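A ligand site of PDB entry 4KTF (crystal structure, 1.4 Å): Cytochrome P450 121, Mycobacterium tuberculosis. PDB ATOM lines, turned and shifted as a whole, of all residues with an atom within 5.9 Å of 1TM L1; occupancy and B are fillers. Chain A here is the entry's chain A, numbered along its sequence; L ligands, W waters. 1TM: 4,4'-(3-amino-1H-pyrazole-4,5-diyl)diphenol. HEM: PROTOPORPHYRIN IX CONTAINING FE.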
ATOM      1  N   THR A  76      36.183 -18.479  -3.508  1.00  0.00           N
ATOM      2  CA  THR A  76      36.542 -17.369  -2.655  1.00  0.00           C
ATOM      3  C   THR A  76      36.175 -17.588  -1.192  1.00  0.00           C
ATOM      4  O   THR A  76      36.295 -16.712  -0.347  1.00  0.00           O
ATOM      5  CB  THR A  76      35.998 -16.027  -3.122  1.00  0.00           C
ATOM      6  OG1 THR A  76      34.572 -16.110  -3.100  1.00  0.00           O
ATOM      7  CG2 THR A  76      36.384 -15.817  -4.590  1.00  0.00           C
ATOM      8  N   VAL A  77      35.669 -18.775  -0.911  1.00  0.00           N
ATOM      9  CA  VAL A  77      35.251 -19.221   0.464  1.00  0.00           C
ATOM     10  C   VAL A  77      35.934 -20.522   0.713  1.00  0.00           C
ATOM     11  O   VAL A  77      36.308 -21.254  -0.213  1.00  0.00           O
ATOM     12  CB  VAL A  77      33.706 -19.407   0.594  1.00  0.00           C
ATOM     13  CG1 VAL A  77      32.997 -18.084   0.434  1.00  0.00           C
ATOM     14  CG2 VAL A  77      33.107 -20.405  -0.374  1.00  0.00           C
ATOM     15  N   VAL A  81      32.186 -24.249   3.042  1.00  0.00           N
ATOM     16  CA  VAL A  81      31.169 -23.180   3.011  1.00  0.00           C
ATOM     17  C   VAL A  81      30.269 -23.280   1.799  1.00  0.00           C
ATOM     18  O   VAL A  81      29.174 -22.716   1.750  1.00  0.00           O
ATOM     19  CB  VAL A  81      31.845 -21.811   3.183  1.00  0.00           C
ATOM     20  CG1 VAL A  81      30.840 -20.649   3.082  1.00  0.00           C
ATOM     21  CG2 VAL A  81      32.544 -21.714   4.509  1.00  0.00           C
ATOM     22  N   VAL A  82      30.684 -23.959   0.742  1.00  0.00           N
ATOM     23  CA  VAL A  82      29.764 -24.218  -0.385  1.00  0.00           C
ATOM     24  C   VAL A  82      28.553 -24.954   0.107  1.00  0.00           C
ATOM     25  O   VAL A  82      27.455 -24.757  -0.462  1.00  0.00           O
ATOM     26  CB  VAL A  82      30.593 -24.903  -1.535  1.00  0.00           C
ATOM     27  CG1 VAL A  82      29.636 -25.308  -2.665  1.00  0.00           C
ATOM     28  CG2 VAL A  82      31.772 -23.984  -2.008  1.00  0.00           C
ATOM     29  N   ASN A  84      27.025 -24.363   2.908  1.00  0.00           N
ATOM     30  CA  ASN A  84      26.600 -23.544   4.062  1.00  0.00           C
ATOM     31  C   ASN A  84      25.235 -23.866   4.515  1.00  0.00           C
ATOM     32  O   ASN A  84      25.059 -24.069   5.714  1.00  0.00           O
ATOM     33  CB  ASN A  84      26.750 -22.130   3.654  1.00  0.00           C
ATOM     34  CG  ASN A  84      26.733 -21.094   4.786  1.00  0.00           C
ATOM     35  OD1 ASN A  84      27.236 -21.327   5.902  1.00  0.00           O
ATOM     36  ND2 ASN A  84      26.186 -19.893   4.466  1.00  0.00           N
ATOM     37  N   MET A  85      24.263 -24.040   3.633  1.00  0.00           N
ATOM     38  CA  MET A  85      22.922 -24.334   4.120  1.00  0.00           C
ATOM     39  C   MET A  85      22.796 -25.725   4.713  1.00  0.00           C
ATOM     40  O   MET A  85      22.054 -25.951   5.694  1.00  0.00           O
ATOM     41  CB  MET A  85      21.853 -24.021   3.054  1.00  0.00           C
ATOM     42  CG  MET A  85      21.507 -22.527   2.957  1.00  0.00           C
ATOM     43  SD  MET A  85      20.840 -21.553   4.344  1.00  0.00           S
ATOM     44  CE  MET A  85      19.821 -22.797   5.117  1.00  0.00           C
ATOM     45  N   SER A 162      34.595  -5.470   1.360  1.00  0.00           N
ATOM     46  CA  SER A 162      35.095  -6.764   0.995  1.00  0.00           C
ATOM     47  C   SER A 162      34.432  -7.309  -0.269  1.00  0.00           C
ATOM     48  O   SER A 162      35.008  -8.224  -0.980  1.00  0.00           O
ATOM     49  CB  SER A 162      34.771  -7.732   2.101  1.00  0.00           C
ATOM     50  OG  SER A 162      35.541  -7.466   3.254  1.00  0.00           O
ATOM     51  N   LEU A 163      33.243  -6.861  -0.641  1.00  0.00           N
ATOM     52  CA  LEU A 163      32.438  -7.576  -1.579  1.00  0.00           C
ATOM     53  C   LEU A 163      32.804  -7.535  -3.058  1.00  0.00           C
ATOM     54  O   LEU A 163      32.559  -8.443  -3.833  1.00  0.00           O
ATOM     55  CB  LEU A 163      30.957  -7.286  -1.414  1.00  0.00           C
ATOM     56  CG  LEU A 163      30.462  -7.526   0.038  1.00  0.00           C
ATOM     57  CD1 LEU A 163      28.964  -7.234   0.156  1.00  0.00           C
ATOM     58  CD2 LEU A 163      30.694  -8.870   0.534  1.00  0.00           C
ATOM     59  N   ALA A 166      35.038 -10.489  -2.865  1.00  0.00           N
ATOM     60  CA  ALA A 166      34.398 -11.709  -2.435  1.00  0.00           C
ATOM     61  C   ALA A 166      33.502 -12.342  -3.435  1.00  0.00           C
ATOM     62  O   ALA A 166      33.436 -13.565  -3.505  1.00  0.00           O
ATOM     63  CB  ALA A 166      33.532 -11.382  -1.201  1.00  0.00           C
ATOM     64  N   PHE A 167      32.840 -11.522  -4.244  1.00  0.00           N
ATOM     65  CA  PHE A 167      31.975 -12.040  -5.287  1.00  0.00           C
ATOM     66  C   PHE A 167      32.569 -11.970  -6.669  1.00  0.00           C
ATOM     67  O   PHE A 167      31.854 -12.073  -7.700  1.00  0.00           O
ATOM     68  CB  PHE A 167      30.604 -11.370  -5.186  1.00  0.00           C
ATOM     69  CG  PHE A 167      29.804 -11.993  -4.074  1.00  0.00           C
ATOM     70  CD1 PHE A 167      29.079 -13.154  -4.278  1.00  0.00           C
ATOM     71  CD2 PHE A 167      29.870 -11.439  -2.782  1.00  0.00           C
ATOM     72  CE1 PHE A 167      28.385 -13.692  -3.178  1.00  0.00           C
ATOM     73  CE2 PHE A 167      29.147 -12.012  -1.705  1.00  0.00           C
ATOM     74  CZ  PHE A 167      28.477 -13.160  -1.974  1.00  0.00           C
ATOM     75  N   MET A 168      33.913 -11.951  -6.757  1.00  0.00           N
ATOM     76  CA  MET A 168      34.557 -12.189  -8.055  1.00  0.00           C
ATOM     77  C   MET A 168      34.293 -13.592  -8.603  1.00  0.00           C
ATOM     78  O   MET A 168      34.017 -14.503  -7.843  1.00  0.00           O
ATOM     79  CB  MET A 168      36.108 -11.946  -7.956  1.00  0.00           C
ATOM     80  CG  MET A 168      36.454 -10.493  -8.020  1.00  0.00           C
ATOM     81  SD  MET A 168      38.193 -10.204  -7.797  1.00  0.00           S
ATOM     82  CE  MET A 168      38.346  -8.433  -8.117  1.00  0.00           C
ATOM     83  N   TRP A 181      38.260 -12.415   4.078  1.00  0.00           N
ATOM     84  CA  TRP A 181      37.465 -13.508   4.733  1.00  0.00           C
ATOM     85  C   TRP A 181      37.920 -13.618   6.134  1.00  0.00           C
ATOM     86  O   TRP A 181      37.120 -13.628   7.142  1.00  0.00           O
ATOM     87  CB  TRP A 181      37.593 -14.809   4.004  1.00  0.00           C
ATOM     88  CG  TRP A 181      36.901 -15.975   4.647  1.00  0.00           C
ATOM     89  CD1 TRP A 181      37.448 -16.838   5.542  1.00  0.00           C
ATOM     90  CD2 TRP A 181      35.525 -16.284   4.553  1.00  0.00           C
ATOM     91  NE1 TRP A 181      36.494 -17.783   5.923  1.00  0.00           N
ATOM     92  CE2 TRP A 181      35.296 -17.428   5.325  1.00  0.00           C
ATOM     93  CE3 TRP A 181      34.450 -15.766   3.824  1.00  0.00           C
ATOM     94  CZ2 TRP A 181      34.054 -18.024   5.446  1.00  0.00           C
ATOM     95  CZ3 TRP A 181      33.190 -16.405   3.905  1.00  0.00           C
ATOM     96  CH2 TRP A 181      33.002 -17.533   4.722  1.00  0.00           C
ATOM     97  N   ASP A 184      36.866 -10.647   8.290  1.00  0.00           N
ATOM     98  CA  ASP A 184      35.450 -10.534   8.451  1.00  0.00           C
ATOM     99  C   ASP A 184      34.930 -11.656   9.380  1.00  0.00           C
ATOM    100  O   ASP A 184      34.030 -11.381  10.209  1.00  0.00           O
ATOM    101  CB  ASP A 184      34.697 -10.520   7.175  1.00  0.00           C
ATOM    102  CG  ASP A 184      35.000  -9.298   6.377  1.00  0.00           C
ATOM    103  OD1 ASP A 184      35.521  -8.293   6.880  1.00  0.00           O
ATOM    104  OD2 ASP A 184      34.666  -9.300   5.129  1.00  0.00           O
ATOM    105  N   VAL A 227      28.995 -13.789   8.234  1.00  0.00           N
ATOM    106  CA  VAL A 227      29.744 -13.260   7.073  1.00  0.00           C
ATOM    107  C   VAL A 227      29.002 -13.567   5.802  1.00  0.00           C
ATOM    108  O   VAL A 227      28.876 -12.639   4.927  1.00  0.00           O
ATOM    109  CB  VAL A 227      31.186 -13.824   7.071  1.00  0.00           C
ATOM    110  CG1 VAL A 227      31.827 -13.433   5.776  1.00  0.00           C
ATOM    111  CG2 VAL A 227      31.985 -13.458   8.313  1.00  0.00           C
ATOM    112  N   THR A 228      28.565 -14.802   5.633  1.00  0.00           N
ATOM    113  CA  THR A 228      27.979 -15.231   4.382  1.00  0.00           C
ATOM    114  C   THR A 228      26.619 -14.629   4.150  1.00  0.00           C
ATOM    115  O   THR A 228      26.232 -14.265   2.993  1.00  0.00           O
ATOM    116  CB  THR A 228      27.856 -16.744   4.280  1.00  0.00           C
ATOM    117  OG1 THR A 228      27.104 -17.275   5.400  1.00  0.00           O
ATOM    118  CG2 THR A 228      29.238 -17.367   4.191  1.00  0.00           C
ATOM    119  N   PHE A 229      25.771 -14.486   5.212  1.00  0.00           N
ATOM    120  CA  PHE A 229      24.446 -13.897   5.040  1.00  0.00           C
ATOM    121  C   PHE A 229      24.554 -12.393   4.778  1.00  0.00           C
ATOM    122  O   PHE A 229      23.845 -11.884   3.918  1.00  0.00           O
ATOM    123  CB  PHE A 229      23.439 -14.272   6.182  1.00  0.00           C
ATOM    124  CG  PHE A 229      22.806 -15.576   5.957  1.00  0.00           C
ATOM    125  CD1 PHE A 229      23.559 -16.752   5.922  1.00  0.00           C
ATOM    126  CD2 PHE A 229      21.416 -15.730   5.688  1.00  0.00           C
ATOM    127  CE1 PHE A 229      22.972 -17.953   5.624  1.00  0.00           C
ATOM    128  CE2 PHE A 229      20.865 -16.978   5.434  1.00  0.00           C
ATOM    129  CZ  PHE A 229      21.632 -18.049   5.464  1.00  0.00           C
ATOM    130  N   GLY A 231      27.129 -10.997   3.219  1.00  0.00           N
ATOM    131  CA  GLY A 231      27.683 -10.799   1.849  1.00  0.00           C
ATOM    132  C   GLY A 231      26.716 -11.195   0.778  1.00  0.00           C
ATOM    133  O   GLY A 231      26.485 -10.405  -0.132  1.00  0.00           O
ATOM    134  N   ALA A 232      26.091 -12.354   0.884  1.00  0.00           N
ATOM    135  CA  ALA A 232      25.144 -12.751  -0.098  1.00  0.00           C
ATOM    136  C   ALA A 232      23.937 -11.833  -0.166  1.00  0.00           C
ATOM    137  O   ALA A 232      23.517 -11.445  -1.247  1.00  0.00           O
ATOM    138  CB  ALA A 232      24.701 -14.148   0.105  1.00  0.00           C
ATOM    139  N   GLN A 384      30.417 -12.291 -10.072  1.00  0.00           N
ATOM    140  CA  GLN A 384      29.288 -13.160  -9.997  1.00  0.00           C
ATOM    141  C   GLN A 384      27.956 -12.412 -10.222  1.00  0.00           C
ATOM    142  O   GLN A 384      26.942 -13.126 -10.325  1.00  0.00           O
ATOM    143  CB  GLN A 384      29.281 -13.885  -8.607  1.00  0.00           C
ATOM    144  CG  GLN A 384      30.452 -14.818  -8.369  1.00  0.00           C
ATOM    145  CD  GLN A 384      30.461 -15.488  -7.035  1.00  0.00           C
ATOM    146  OE1 GLN A 384      31.559 -15.480  -6.326  1.00  0.00           O
ATOM    147  NE2 GLN A 384      29.407 -16.001  -6.570  1.00  0.00           N
HETATM  148  CAO 1TM L   1      28.963 -18.774  -0.618  1.00  0.00           C
HETATM  149  CAP 1TM L   1      28.010 -19.516   0.154  1.00  0.00           C
HETATM  150  CAQ 1TM L   1      26.948 -18.864   0.730  1.00  0.00           C
HETATM  151  OAT 1TM L   1      25.978 -19.636   1.422  1.00  0.00           O
HETATM  152  CAR 1TM L   1      26.861 -17.512   0.670  1.00  0.00           C
HETATM  153  CAS 1TM L   1      27.857 -16.806  -0.103  1.00  0.00           C
HETATM  154  CAN 1TM L   1      28.893 -17.422  -0.764  1.00  0.00           C
HETATM  155  CAJ 1TM L   1      29.888 -16.728  -1.556  1.00  0.00           C
HETATM  156  CAK 1TM L   1      30.088 -16.990  -2.935  1.00  0.00           C
HETATM  157  NAM 1TM L   1      29.363 -17.945  -3.733  1.00  0.00           N
HETATM  158  NAL 1TM L   1      31.056 -16.214  -3.481  1.00  0.00           N
HETATM  159  NAA 1TM L   1      31.435 -15.496  -2.410  1.00  0.00           N
HETATM  160  CAB 1TM L   1      30.815 -15.780  -1.246  1.00  0.00           C
HETATM  161  CAC 1TM L   1      31.203 -14.977  -0.117  1.00  0.00           C
HETATM  162  CAD 1TM L   1      32.530 -14.653   0.086  1.00  0.00           C
HETATM  163  CAE 1TM L   1      32.956 -13.832   1.085  1.00  0.00           C
HETATM  164  CAF 1TM L   1      32.030 -13.246   1.943  1.00  0.00           C
HETATM  165  OAI 1TM L   1      32.500 -12.346   2.832  1.00  0.00           O
HETATM  166  CAG 1TM L   1      30.653 -13.610   1.837  1.00  0.00           C
HETATM  167  CAH 1TM L   1      30.285 -14.438   0.817  1.00  0.00           C
HETATM  168  CHA HEM L   2      20.803 -18.599  -2.682  1.00  0.00           C
HETATM  169  CHB HEM L   2      19.167 -15.111  -5.578  1.00  0.00           C
HETATM  170  CHC HEM L   2      18.751 -12.194  -1.682  1.00  0.00           C
HETATM  171  CHD HEM L   2      21.134 -15.401   0.875  1.00  0.00           C
HETATM  172  C1A HEM L   2      20.258 -17.916  -3.814  1.00  0.00           C
HETATM  173  C2A HEM L   2      20.048 -18.511  -5.104  1.00  0.00           C
HETATM  174  C3A HEM L   2      19.597 -17.511  -5.959  1.00  0.00           C
HETATM  175  C4A HEM L   2      19.571 -16.300  -5.168  1.00  0.00           C
HETATM  176  CMA HEM L   2      19.347 -17.596  -7.403  1.00  0.00           C
HETATM  177  CAA HEM L   2      20.196 -19.967  -5.442  1.00  0.00           C
HETATM  178  CBA HEM L   2      21.643 -20.384  -5.701  1.00  0.00           C
HETATM  179  CGA HEM L   2      21.758 -21.751  -6.235  1.00  0.00           C
HETATM  180  O1A HEM L   2      20.779 -22.584  -6.134  1.00  0.00           O
HETATM  181  O2A HEM L   2      22.882 -22.186  -6.723  1.00  0.00           O
HETATM  182  C1B HEM L   2      18.961 -13.950  -4.783  1.00  0.00           C
HETATM  183  C2B HEM L   2      18.361 -12.710  -5.231  1.00  0.00           C
HETATM  184  C3B HEM L   2      18.242 -11.919  -4.134  1.00  0.00           C
HETATM  185  C4B HEM L   2      18.768 -12.659  -2.987  1.00  0.00           C
HETATM  186  CMB HEM L   2      18.007 -12.454  -6.660  1.00  0.00           C
HETATM  187  CAB HEM L   2      17.728 -10.513  -4.014  1.00  0.00           C
HETATM  188  CBB HEM L   2      16.846 -10.012  -4.865  1.00  0.00           C
HETATM  189  C1C HEM L   2      19.286 -12.831  -0.610  1.00  0.00           C
HETATM  190  C2C HEM L   2      19.296 -12.325   0.731  1.00  0.00           C
HETATM  191  C3C HEM L   2      20.051 -13.197   1.430  1.00  0.00           C
HETATM  192  C4C HEM L   2      20.409 -14.305   0.588  1.00  0.00           C
HETATM  193  CMC HEM L   2      18.705 -11.066   1.201  1.00  0.00           C
HETATM  194  CAC HEM L   2      20.375 -13.189   2.871  1.00  0.00           C
HETATM  195  CBC HEM L   2      20.149 -12.334   3.769  1.00  0.00           C
HETATM  196  C1D HEM L   2      21.391 -16.501   0.096  1.00  0.00           C
HETATM  197  C2D HEM L   2      22.097 -17.725   0.559  1.00  0.00           C
HETATM  198  C3D HEM L   2      21.970 -18.638  -0.441  1.00  0.00           C
HETATM  199  C4D HEM L   2      21.176 -17.960  -1.498  1.00  0.00           C
HETATM  200  CMD HEM L   2      22.768 -17.860   1.874  1.00  0.00           C
HETATM  201  CAD HEM L   2      22.451 -20.040  -0.557  1.00  0.00           C
HETATM  202  CBD HEM L   2      21.343 -21.069  -0.219  1.00  0.00           C
HETATM  203  CGD HEM L   2      21.851 -22.506  -0.326  1.00  0.00           C
HETATM  204  O1D HEM L   2      20.962 -23.441  -0.218  1.00  0.00           O
HETATM  205  O2D HEM L   2      23.090 -22.758  -0.411  1.00  0.00           O
HETATM  206  NA  HEM L   2      19.911 -16.592  -3.831  1.00  0.00           N
HETATM  207  NB  HEM L   2      19.092 -13.830  -3.460  1.00  0.00           N
HETATM  208  NC  HEM L   2      19.878 -14.044  -0.708  1.00  0.00           N
HETATM  209  ND  HEM L   2      20.754 -16.727  -1.094  1.00  0.00           N
HETATM  210 FE   HEM L   2      19.853 -15.342  -2.229  1.00  0.00          FE
HETATM  211  O   HOH W   1      35.040 -11.380   3.220  1.00  0.00           O
HETATM  212  O   HOH W   2      28.390 -19.018  -6.625  1.00  0.00           O
HETATM  213  O   HOH W   3      31.103 -20.315  -3.672  1.00  0.00           O
HETATM  214  O   HOH W   4      25.434 -22.020   0.431  1.00  0.00           O
HETATM  215  O   HOH W   5      30.535 -10.720   3.741  1.00  0.00           O
HETATM  216  O   HOH W   6      33.362 -18.670  -3.995  1.00  0.00           O
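Val 77 touches 1TM L1 (CG1 to CAD, 3.5 Å). Val 81 touches 1TM L1. Phe 167 touches 1TM L1 (CZ to CAH, 3.6 Å). CE3 of Trp 181 touches CAE of 1TM L1, at 3.7 Å. Val 227 touches 1TM L1. Thr 228 touches 1TM L1 (CB to CAR, 3.8 Å). Hydrophobic or aromatic side chains within 4 Å of 1TM L1: Val 77, Ala 166, Phe 167, Trp 181 and Val 227. Of the 19 residues printed, 10 come within 4 Å of 1TM L1. The nearest printed residue that does not touch 1TM L1 is Ala 232 (4.04 Å).
A nitrogen (NAL) of 1TM L1 sits close to the side-chain amide oxygen (OE1) of Gln 384, 3.0 Å away. NAA of 1TM L1 sits at hydrogen-bond distance from O of Ala 166 (3.0 Å). The side-chain amide nitrogen (ND2) of Asn 84 sits at hydrogen-bond distance from an oxygen (OAT) of 1TM L1 (3.1 Å). The side-chain hydroxyl (OG1) of Thr 76 sits at hydrogen-bond distance from a nitrogen (NAA) of 1TM L1, at 3.3 Å.
N of Gln 384 lies within hydrogen-bond range of O of Phe 167 (2.8 Å). The backbone carbonyl oxygen (O) of Met 168 sits close to the side-chain amide oxygen (OE1) of Gln 384, 3.0 Å away. OG1 of Thr 76 is in hydrogen-bond range of O of Ala 166 (2.8 Å). ND2 of Asn 84 sits at hydrogen-bond distance from OG1 of Thr 228, 2.9 Å away.
Water W4 bridges an oxygen (O2D) of HEM L2 and an oxygen (OAT) of 1TM L1. Water W5 lies within hydrogen-bond range of an oxygen (OAI) of 1TM L1 (2.7 Å), the backbone carbonyl oxygen of Val 227 (2.8 Å) and the backbone NH of Gly 231 (3.5 Å). Water W1 lies within hydrogen-bond range of OAI of 1TM L1, OD2 of Asp 184 and N of Trp 181. Water W2 lies within hydrogen-bond range of the side-chain amide nitrogen (NE2) of Gln 384 (3.2 Å) and a nitrogen (NAM) of 1TM L1 (3.2 Å). Water W6 lies within hydrogen-bond range of N of Thr 76 (2.9 Å) and NAL of 1TM L1 (3.4 Å).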
